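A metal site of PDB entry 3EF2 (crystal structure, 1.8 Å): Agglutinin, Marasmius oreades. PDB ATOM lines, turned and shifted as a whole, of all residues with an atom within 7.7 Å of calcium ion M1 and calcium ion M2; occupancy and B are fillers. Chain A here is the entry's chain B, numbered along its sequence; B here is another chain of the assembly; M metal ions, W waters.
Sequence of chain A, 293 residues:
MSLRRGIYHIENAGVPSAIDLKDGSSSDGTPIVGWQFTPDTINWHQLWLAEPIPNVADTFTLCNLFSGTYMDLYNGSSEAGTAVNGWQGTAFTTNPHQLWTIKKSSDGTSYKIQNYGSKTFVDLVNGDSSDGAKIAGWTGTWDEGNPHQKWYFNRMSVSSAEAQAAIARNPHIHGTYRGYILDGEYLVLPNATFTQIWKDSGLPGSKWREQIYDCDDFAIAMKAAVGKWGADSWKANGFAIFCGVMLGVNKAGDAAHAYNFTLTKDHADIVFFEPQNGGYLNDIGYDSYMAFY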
ATOM      1  N   TRP A 208     -18.069   6.061 -21.581  1.00  0.00           N
ATOM      2  CA  TRP A 208     -17.858   4.621 -21.408  1.00  0.00           C
ATOM      3  C   TRP A 208     -19.170   3.880 -21.706  1.00  0.00           C
ATOM      4  O   TRP A 208     -20.224   4.208 -21.149  1.00  0.00           O
ATOM      5  CB  TRP A 208     -17.378   4.288 -19.970  1.00  0.00           C
ATOM      6  CG  TRP A 208     -16.909   2.853 -19.823  1.00  0.00           C
ATOM      7  CD1 TRP A 208     -15.617   2.411 -19.940  1.00  0.00           C
ATOM      8  CD2 TRP A 208     -17.711   1.686 -19.574  1.00  0.00           C
ATOM      9  NE1 TRP A 208     -15.568   1.047 -19.739  1.00  0.00           N
ATOM     10  CE2 TRP A 208     -16.836   0.580 -19.527  1.00  0.00           C
ATOM     11  CE3 TRP A 208     -19.087   1.478 -19.385  1.00  0.00           C
ATOM     12  CZ2 TRP A 208     -17.288  -0.733 -19.288  1.00  0.00           C
ATOM     13  CZ3 TRP A 208     -19.540   0.158 -19.134  1.00  0.00           C
ATOM     14  CH2 TRP A 208     -18.640  -0.918 -19.101  1.00  0.00           C
ATOM     15  N   ARG A 209     -19.108   2.872 -22.578  1.00  0.00           N
ATOM     16  CA  ARG A 209     -20.288   2.076 -22.957  1.00  0.00           C
ATOM     17  C   ARG A 209     -19.890   0.610 -23.081  1.00  0.00           C
ATOM     18  O   ARG A 209     -18.900   0.283 -23.730  1.00  0.00           O
ATOM     19  CB  ARG A 209     -20.864   2.557 -24.301  1.00  0.00           C
ATOM     20  CG  ARG A 209     -21.408   4.004 -24.283  1.00  0.00           C
ATOM     21  CD  ARG A 209     -21.742   4.494 -25.708  1.00  0.00           C
ATOM     22  NE  ARG A 209     -22.703   3.604 -26.357  1.00  0.00           N
ATOM     23  CZ  ARG A 209     -23.026   3.609 -27.655  1.00  0.00           C
ATOM     24  NH1 ARG A 209     -22.451   4.449 -28.499  1.00  0.00           N
ATOM     25  NH2 ARG A 209     -23.911   2.733 -28.106  1.00  0.00           N
ATOM     26  N   GLU A 210     -20.678  -0.249 -22.459  1.00  0.00           N
ATOM     27  CA  GLU A 210     -20.377  -1.681 -22.366  1.00  0.00           C
ATOM     28  C   GLU A 210     -20.050  -2.278 -23.744  1.00  0.00           C
ATOM     29  O   GLU A 210     -20.901  -2.235 -24.639  1.00  0.00           O
ATOM     30  CB  GLU A 210     -21.593  -2.380 -21.755  1.00  0.00           C
ATOM     31  CG  GLU A 210     -21.495  -3.866 -21.507  1.00  0.00           C
ATOM     32  CD  GLU A 210     -22.877  -4.490 -21.257  1.00  0.00           C
ATOM     33  OE1 GLU A 210     -23.808  -3.745 -20.836  1.00  0.00           O
ATOM     34  OE2 GLU A 210     -23.051  -5.699 -21.531  1.00  0.00           O
ATOM     35  N   GLN A 211     -18.823  -2.791 -23.870  1.00  0.00           N
ATOM     36  CA  GLN A 211     -18.233  -3.380 -25.102  1.00  0.00           C
ATOM     37  C   GLN A 211     -18.004  -2.457 -26.312  1.00  0.00           C
ATOM     38  O   GLN A 211     -16.949  -2.501 -26.954  1.00  0.00           O
ATOM     39  CB  GLN A 211     -18.987  -4.647 -25.529  1.00  0.00           C
ATOM     40  CG  GLN A 211     -18.978  -5.760 -24.447  1.00  0.00           C
ATOM     41  CD  GLN A 211     -19.315  -7.137 -25.015  1.00  0.00           C
ATOM     42  OE1 GLN A 211     -18.779  -7.557 -26.042  1.00  0.00           O
ATOM     43  NE2 GLN A 211     -20.223  -7.849 -24.333  1.00  0.00           N
ATOM     44  N   ILE A 212     -19.022  -1.634 -26.611  1.00  0.00           N
ATOM     45  CA  ILE A 212     -19.060  -0.842 -27.856  1.00  0.00           C
ATOM     46  C   ILE A 212     -18.115   0.368 -27.776  1.00  0.00           C
ATOM     47  O   ILE A 212     -17.571   0.822 -28.795  1.00  0.00           O
ATOM     48  CB  ILE A 212     -20.547  -0.444 -28.210  1.00  0.00           C
ATOM     49  CG1 ILE A 212     -20.677   0.097 -29.663  1.00  0.00           C
ATOM     50  CG2 ILE A 212     -21.116   0.501 -27.168  1.00  0.00           C
ATOM     51  CD1 ILE A 212     -20.332  -0.956 -30.790  1.00  0.00           C
ATOM     52  N   TYR A 213     -17.889   0.853 -26.558  1.00  0.00           N
ATOM     53  CA  TYR A 213     -16.834   1.872 -26.352  1.00  0.00           C
ATOM     54  C   TYR A 213     -16.359   1.835 -24.912  1.00  0.00           C
ATOM     55  O   TYR A 213     -16.686   2.725 -24.100  1.00  0.00           O
ATOM     56  CB  TYR A 213     -17.252   3.269 -26.785  1.00  0.00           C
ATOM     57  CG  TYR A 213     -16.080   4.018 -27.371  1.00  0.00           C
ATOM     58  CD1 TYR A 213     -15.330   4.891 -26.578  1.00  0.00           C
ATOM     59  CD2 TYR A 213     -15.666   3.794 -28.690  1.00  0.00           C
ATOM     60  CE1 TYR A 213     -14.218   5.549 -27.088  1.00  0.00           C
ATOM     61  CE2 TYR A 213     -14.556   4.459 -29.236  1.00  0.00           C
ATOM     62  CZ  TYR A 213     -13.841   5.351 -28.420  1.00  0.00           C
ATOM     63  OH  TYR A 213     -12.728   6.009 -28.929  1.00  0.00           O
ATOM     64  N   ASP A 214     -15.641   0.760 -24.586  1.00  0.00           N
ATOM     65  CA  ASP A 214     -15.221   0.495 -23.203  1.00  0.00           C
ATOM     66  C   ASP A 214     -13.691   0.615 -23.102  1.00  0.00           C
ATOM     67  O   ASP A 214     -13.097   1.273 -23.949  1.00  0.00           O
ATOM     68  CB  ASP A 214     -15.790  -0.836 -22.678  1.00  0.00           C
ATOM     69  CG  ASP A 214     -15.290  -2.069 -23.430  1.00  0.00           C
ATOM     70  OD1 ASP A 214     -14.824  -1.972 -24.586  1.00  0.00           O
ATOM     71  OD2 ASP A 214     -15.367  -3.156 -22.831  1.00  0.00           O
ATOM     72  N   OCS A 215     -13.075  -0.006 -22.101  1.00  0.00           N
ATOM     73  CA  OCS A 215     -11.634   0.176 -21.784  1.00  0.00           C
ATOM     74  CB  OCS A 215     -11.181  -0.905 -20.762  1.00  0.00           C
ATOM     75  SG  OCS A 215     -12.273  -1.050 -19.352  1.00  0.00           S
ATOM     76  C   OCS A 215     -10.752   0.077 -23.031  1.00  0.00           C
ATOM     77  O   OCS A 215      -9.940   0.961 -23.315  1.00  0.00           O
ATOM     78  OD1 OCS A 215     -13.542  -1.570 -19.736  1.00  0.00           O
ATOM     79  OD2 OCS A 215     -12.398   0.260 -18.841  1.00  0.00           O
ATOM     80  OD3 OCS A 215     -11.697  -1.924 -18.372  1.00  0.00           O
ATOM     81  N   ASP A 216     -10.901  -1.027 -23.755  1.00  0.00           N
ATOM     82  CA  ASP A 216     -10.074  -1.307 -24.918  1.00  0.00           C
ATOM     83  C   ASP A 216     -10.145  -0.190 -25.977  1.00  0.00           C
ATOM     84  O   ASP A 216      -9.139   0.186 -26.582  1.00  0.00           O
ATOM     85  CB  ASP A 216     -10.373  -2.724 -25.482  1.00  0.00           C
ATOM     86  CG  ASP A 216     -11.862  -2.902 -25.905  1.00  0.00           C
ATOM     87  OD1 ASP A 216     -12.720  -3.391 -25.145  1.00  0.00           O
ATOM     88  OD2 ASP A 216     -12.207  -2.548 -27.026  1.00  0.00           O
ATOM     89  N   ASP A 217     -11.340   0.348 -26.191  1.00  0.00           N
ATOM     90  CA  ASP A 217     -11.567   1.371 -27.211  1.00  0.00           C
ATOM     91  C   ASP A 217     -10.860   2.665 -26.835  1.00  0.00           C
ATOM     92  O   ASP A 217     -10.220   3.295 -27.688  1.00  0.00           O
ATOM     93  CB  ASP A 217     -13.081   1.574 -27.407  1.00  0.00           C
ATOM     94  CG  ASP A 217     -13.754   0.270 -27.820  1.00  0.00           C
ATOM     95  OD1 ASP A 217     -13.555  -0.108 -28.984  1.00  0.00           O
ATOM     96  OD2 ASP A 217     -14.389  -0.406 -26.968  1.00  0.00           O
ATOM     97  N   PHE A 218     -10.950   3.058 -25.561  1.00  0.00           N
ATOM     98  CA  PHE A 218     -10.263   4.280 -25.080  1.00  0.00           C
ATOM     99  C   PHE A 218      -8.745   4.160 -25.251  1.00  0.00           C
ATOM    100  O   PHE A 218      -8.085   5.089 -25.759  1.00  0.00           O
ATOM    101  CB  PHE A 218     -10.603   4.553 -23.616  1.00  0.00           C
ATOM    102  CG  PHE A 218     -11.923   5.250 -23.400  1.00  0.00           C
ATOM    103  CD1 PHE A 218     -11.966   6.636 -23.248  1.00  0.00           C
ATOM    104  CD2 PHE A 218     -13.114   4.522 -23.272  1.00  0.00           C
ATOM    105  CE1 PHE A 218     -13.184   7.311 -23.032  1.00  0.00           C
ATOM    106  CE2 PHE A 218     -14.333   5.176 -23.019  1.00  0.00           C
ATOM    107  CZ  PHE A 218     -14.370   6.575 -22.900  1.00  0.00           C
ATOM    108  N   ILE A 220      -6.924   2.039 -27.223  1.00  0.00           N
ATOM    109  CA  ILE A 220      -6.517   1.970 -28.619  1.00  0.00           C
ATOM    110  C   ILE A 220      -6.673   3.343 -29.288  1.00  0.00           C
ATOM    111  O   ILE A 220      -5.812   3.749 -30.078  1.00  0.00           O
ATOM    112  CB  ILE A 220      -7.260   0.830 -29.372  1.00  0.00           C
ATOM    113  CG1 ILE A 220      -6.584  -0.512 -29.044  1.00  0.00           C
ATOM    114  CG2 ILE A 220      -7.297   1.077 -30.896  1.00  0.00           C
ATOM    115  CD1 ILE A 220      -7.447  -1.749 -29.282  1.00  0.00           C
ATOM    116  N   ALA A 258      -8.025  -2.070 -19.564  1.00  0.00           N
ATOM    117  CA  ALA A 258      -7.113  -1.658 -20.647  1.00  0.00           C
ATOM    118  C   ALA A 258      -6.804  -0.180 -20.454  1.00  0.00           C
ATOM    119  O   ALA A 258      -7.675   0.605 -20.088  1.00  0.00           O
ATOM    120  CB  ALA A 258      -7.736  -1.907 -22.010  1.00  0.00           C
ATOM    121  N   ILE B 181      -8.070 -11.240 -26.312  1.00  0.00           N
ATOM    122  CA  ILE B 181      -9.479 -10.981 -26.577  1.00  0.00           C
ATOM    123  C   ILE B 181      -9.929  -9.767 -25.761  1.00  0.00           C
ATOM    124  O   ILE B 181      -9.693  -9.705 -24.543  1.00  0.00           O
ATOM    125  CB  ILE B 181     -10.323 -12.214 -26.213  1.00  0.00           C
ATOM    126  CG1 ILE B 181      -9.886 -13.404 -27.097  1.00  0.00           C
ATOM    127  CG2 ILE B 181     -11.842 -11.903 -26.316  1.00  0.00           C
ATOM    128  CD1 ILE B 181     -10.550 -14.749 -26.779  1.00  0.00           C
ATOM    129  N   LEU B 182     -10.648  -8.849 -26.424  1.00  0.00           N
ATOM    130  CA  LEU B 182     -10.974  -7.567 -25.807  1.00  0.00           C
ATOM    131  C   LEU B 182     -12.454  -7.394 -25.444  1.00  0.00           C
ATOM    132  O   LEU B 182     -12.797  -6.613 -24.540  1.00  0.00           O
ATOM    133  CB  LEU B 182     -10.510  -6.416 -26.719  1.00  0.00           C
ATOM    134  CG  LEU B 182      -9.030  -6.400 -27.139  1.00  0.00           C
ATOM    135  CD1 LEU B 182      -8.821  -5.289 -28.165  1.00  0.00           C
ATOM    136  CD2 LEU B 182      -8.116  -6.165 -25.942  1.00  0.00           C
ATOM    137  N   ASP B 183     -13.341  -8.114 -26.141  1.00  0.00           N
ATOM    138  CA  ASP B 183     -14.774  -8.003 -25.890  1.00  0.00           C
ATOM    139  C   ASP B 183     -15.431  -9.397 -25.947  1.00  0.00           C
ATOM    140  O   ASP B 183     -14.722 -10.405 -25.958  1.00  0.00           O
ATOM    141  CB  ASP B 183     -15.429  -7.002 -26.876  1.00  0.00           C
ATOM    142  CG  ASP B 183     -14.906  -5.536 -26.696  1.00  0.00           C
ATOM    143  OD1 ASP B 183     -15.062  -4.908 -25.634  1.00  0.00           O
ATOM    144  OD2 ASP B 183     -14.341  -4.975 -27.655  1.00  0.00           O
ATOM    145  N   GLY B 184     -16.757  -9.471 -25.973  1.00  0.00           N
ATOM    146  CA  GLY B 184     -17.448 -10.769 -25.792  1.00  0.00           C
ATOM    147  C   GLY B 184     -18.328 -11.189 -26.961  1.00  0.00           C
ATOM    148  O   GLY B 184     -18.536 -12.387 -27.198  1.00  0.00           O
ATOM    149  N   TYR B 186     -19.516  -9.748 -31.077  1.00  0.00           N
ATOM    150  CA  TYR B 186     -19.119  -8.826 -32.142  1.00  0.00           C
ATOM    151  C   TYR B 186     -20.033  -8.840 -33.379  1.00  0.00           C
ATOM    152  O   TYR B 186     -20.212  -9.888 -33.992  1.00  0.00           O
ATOM    153  CB  TYR B 186     -17.723  -9.185 -32.653  1.00  0.00           C
ATOM    154  CG  TYR B 186     -16.613  -9.182 -31.632  1.00  0.00           C
ATOM    155  CD1 TYR B 186     -15.838  -8.038 -31.434  1.00  0.00           C
ATOM    156  CD2 TYR B 186     -16.317 -10.321 -30.876  1.00  0.00           C
ATOM    157  CE1 TYR B 186     -14.780  -8.023 -30.522  1.00  0.00           C
ATOM    158  CE2 TYR B 186     -15.261 -10.334 -29.947  1.00  0.00           C
ATOM    159  CZ  TYR B 186     -14.504  -9.179 -29.784  1.00  0.00           C
ATOM    160  OH  TYR B 186     -13.457  -9.169 -28.899  1.00  0.00           O
ATOM    161  N   LYS B 223      -8.162  -0.170 -36.634  1.00  0.00           N
ATOM    162  CA  LYS B 223      -8.917  -0.677 -35.475  1.00  0.00           C
ATOM    163  C   LYS B 223      -9.612   0.480 -34.742  1.00  0.00           C
ATOM    164  O   LYS B 223     -10.783   0.351 -34.346  1.00  0.00           O
ATOM    165  CB  LYS B 223      -8.052  -1.488 -34.504  1.00  0.00           C
ATOM    166  CG  LYS B 223      -8.929  -2.161 -33.402  1.00  0.00           C
ATOM    167  CD  LYS B 223      -8.373  -3.477 -32.878  1.00  0.00           C
ATOM    168  CE  LYS B 223      -9.231  -4.013 -31.699  1.00  0.00           C
ATOM    169  NZ  LYS B 223     -10.673  -4.135 -32.015  1.00  0.00           N
ATOM    170  N   GLY B 227     -13.687   1.106 -34.199  1.00  0.00           N
ATOM    171  CA  GLY B 227     -14.209   1.355 -32.837  1.00  0.00           C
ATOM    172  C   GLY B 227     -15.023   2.660 -32.763  1.00  0.00           C
ATOM    173  O   GLY B 227     -16.117   2.676 -32.170  1.00  0.00           O
ATOM    174  N   PHE B 239     -22.146  -5.037 -27.056  1.00  0.00           N
ATOM    175  CA  PHE B 239     -21.508  -5.703 -28.191  1.00  0.00           C
ATOM    176  C   PHE B 239     -20.421  -4.766 -28.741  1.00  0.00           C
ATOM    177  O   PHE B 239     -20.423  -3.543 -28.459  1.00  0.00           O
ATOM    178  CB  PHE B 239     -22.539  -6.026 -29.296  1.00  0.00           C
ATOM    179  CG  PHE B 239     -23.039  -4.782 -29.995  1.00  0.00           C
ATOM    180  CD1 PHE B 239     -23.945  -3.935 -29.363  1.00  0.00           C
ATOM    181  CD2 PHE B 239     -22.531  -4.420 -31.245  1.00  0.00           C
ATOM    182  CE1 PHE B 239     -24.367  -2.741 -29.989  1.00  0.00           C
ATOM    183  CE2 PHE B 239     -22.956  -3.233 -31.884  1.00  0.00           C
ATOM    184  CZ  PHE B 239     -23.854  -2.396 -31.256  1.00  0.00           C
ATOM    185  N   ALA B 240     -19.511  -5.353 -29.521  1.00  0.00           N
ATOM    186  CA  ALA B 240     -18.472  -4.577 -30.226  1.00  0.00           C
ATOM    187  C   ALA B 240     -18.547  -4.863 -31.732  1.00  0.00           C
ATOM    188  O   ALA B 240     -19.364  -5.678 -32.170  1.00  0.00           O
ATOM    189  CB  ALA B 240     -17.068  -4.930 -29.674  1.00  0.00           C
ATOM    190  N   ILE B 241     -17.732  -4.157 -32.518  1.00  0.00           N
ATOM    191  CA  ILE B 241     -17.659  -4.396 -33.967  1.00  0.00           C
ATOM    192  C   ILE B 241     -16.404  -5.215 -34.230  1.00  0.00           C
ATOM    193  O   ILE B 241     -15.331  -4.884 -33.708  1.00  0.00           O
ATOM    194  CB  ILE B 241     -17.595  -3.061 -34.777  1.00  0.00           C
ATOM    195  CG1 ILE B 241     -18.663  -2.032 -34.317  1.00  0.00           C
ATOM    196  CG2 ILE B 241     -17.702  -3.346 -36.299  1.00  0.00           C
ATOM    197  CD1 ILE B 241     -20.110  -2.577 -34.253  1.00  0.00           C
ATOM    198  N   TYR B 293      -8.247  -8.294 -30.616  1.00  0.00           N
ATOM    199  CA  TYR B 293      -9.554  -8.118 -31.247  1.00  0.00           C
ATOM    200  C   TYR B 293     -10.654  -8.174 -30.177  1.00  0.00           C
ATOM    201  O   TYR B 293     -11.747  -7.629 -30.374  1.00  0.00           O
ATOM    202  CB  TYR B 293      -9.814  -9.222 -32.291  1.00  0.00           C
ATOM    203  CG  TYR B 293      -9.727 -10.653 -31.762  1.00  0.00           C
ATOM    204  CD1 TYR B 293      -8.499 -11.339 -31.766  1.00  0.00           C
ATOM    205  CD2 TYR B 293     -10.854 -11.322 -31.292  1.00  0.00           C
ATOM    206  CE1 TYR B 293      -8.399 -12.658 -31.295  1.00  0.00           C
ATOM    207  CE2 TYR B 293     -10.774 -12.650 -30.819  1.00  0.00           C
ATOM    208  CZ  TYR B 293      -9.546 -13.307 -30.840  1.00  0.00           C
ATOM    209  OH  TYR B 293      -9.449 -14.611 -30.385  1.00  0.00           O
ATOM    210  OXT TYR B 293     -10.482  -8.791 -29.144  1.00  0.00           O
HETATM  211 CA    CA M   1     -14.555  -2.775 -26.767  1.00  0.00          CA
HETATM  212 CA    CA M   2     -13.873  -4.782 -23.635  1.00  0.00          CA
HETATM  213  O   HOH W   1     -15.140  -6.311 -22.434  1.00  0.00           O
HETATM  214  O   HOH W   2     -14.520  -2.499 -29.138  1.00  0.00           O
HETATM  215  O   HOH W   3     -12.286  -4.062 -22.083  1.00  0.00           O
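The backbone NH (N) of Leu 182 of chain B lies within hydrogen-bond range of the chain-end carboxylate (OXT) of Tyr 293 of chain B, at 2.7 Å. N of Asp 183 of chain B is in hydrogen-bond range of OH of Tyr 186 of chain B, 3.0 Å away. The side-chain amide oxygen of Gln 211 is in hydrogen-bond range of the backbone NH of Gly 184 of chain B, at 2.8 Å. N of Asp 214 sits at hydrogen-bond distance from O of Arg 209, 3.4 Å away.
Within 4 Å of calcium ion M1: Gln 211, Asp 214, Asp 216, Asp 217 and Asp 183 of chain B.
Of the 24 residues printed, 4 come within 4 Å of calcium ion M2.
Calcium ion M1 is bound by OD1 of Asp 214 (2.3 Å), OD2 of Asp 216 (2.4 Å), OD2 of Asp 183 of chain B (2.4 Å), OD2 of Asp 217 (2.4 Å), water W2 (2.4 Å), O of Gln 211 (2.4 Å), OD1 of Asp 183 of chain B (2.5 Å) and OD1 of Asp 216 (2.5 Å). Calcium ion M1 has eight donor atoms within binding distance.
Calcium ion M2 is bound by O of Leu 182 of chain B (2.3 Å), water W1 (2.3 Å), OD1 of Asp 183 of chain B (2.3 Å), water W3 (2.3 Å), OD2 of Asp 214 (2.3 Å) and OD1 of Asp 216 (2.4 Å). Calcium ion M2 has six donor atoms within binding distance. Slightly farther from calcium ion M2 lies OD1 of Asp 214 (3.1 Å).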
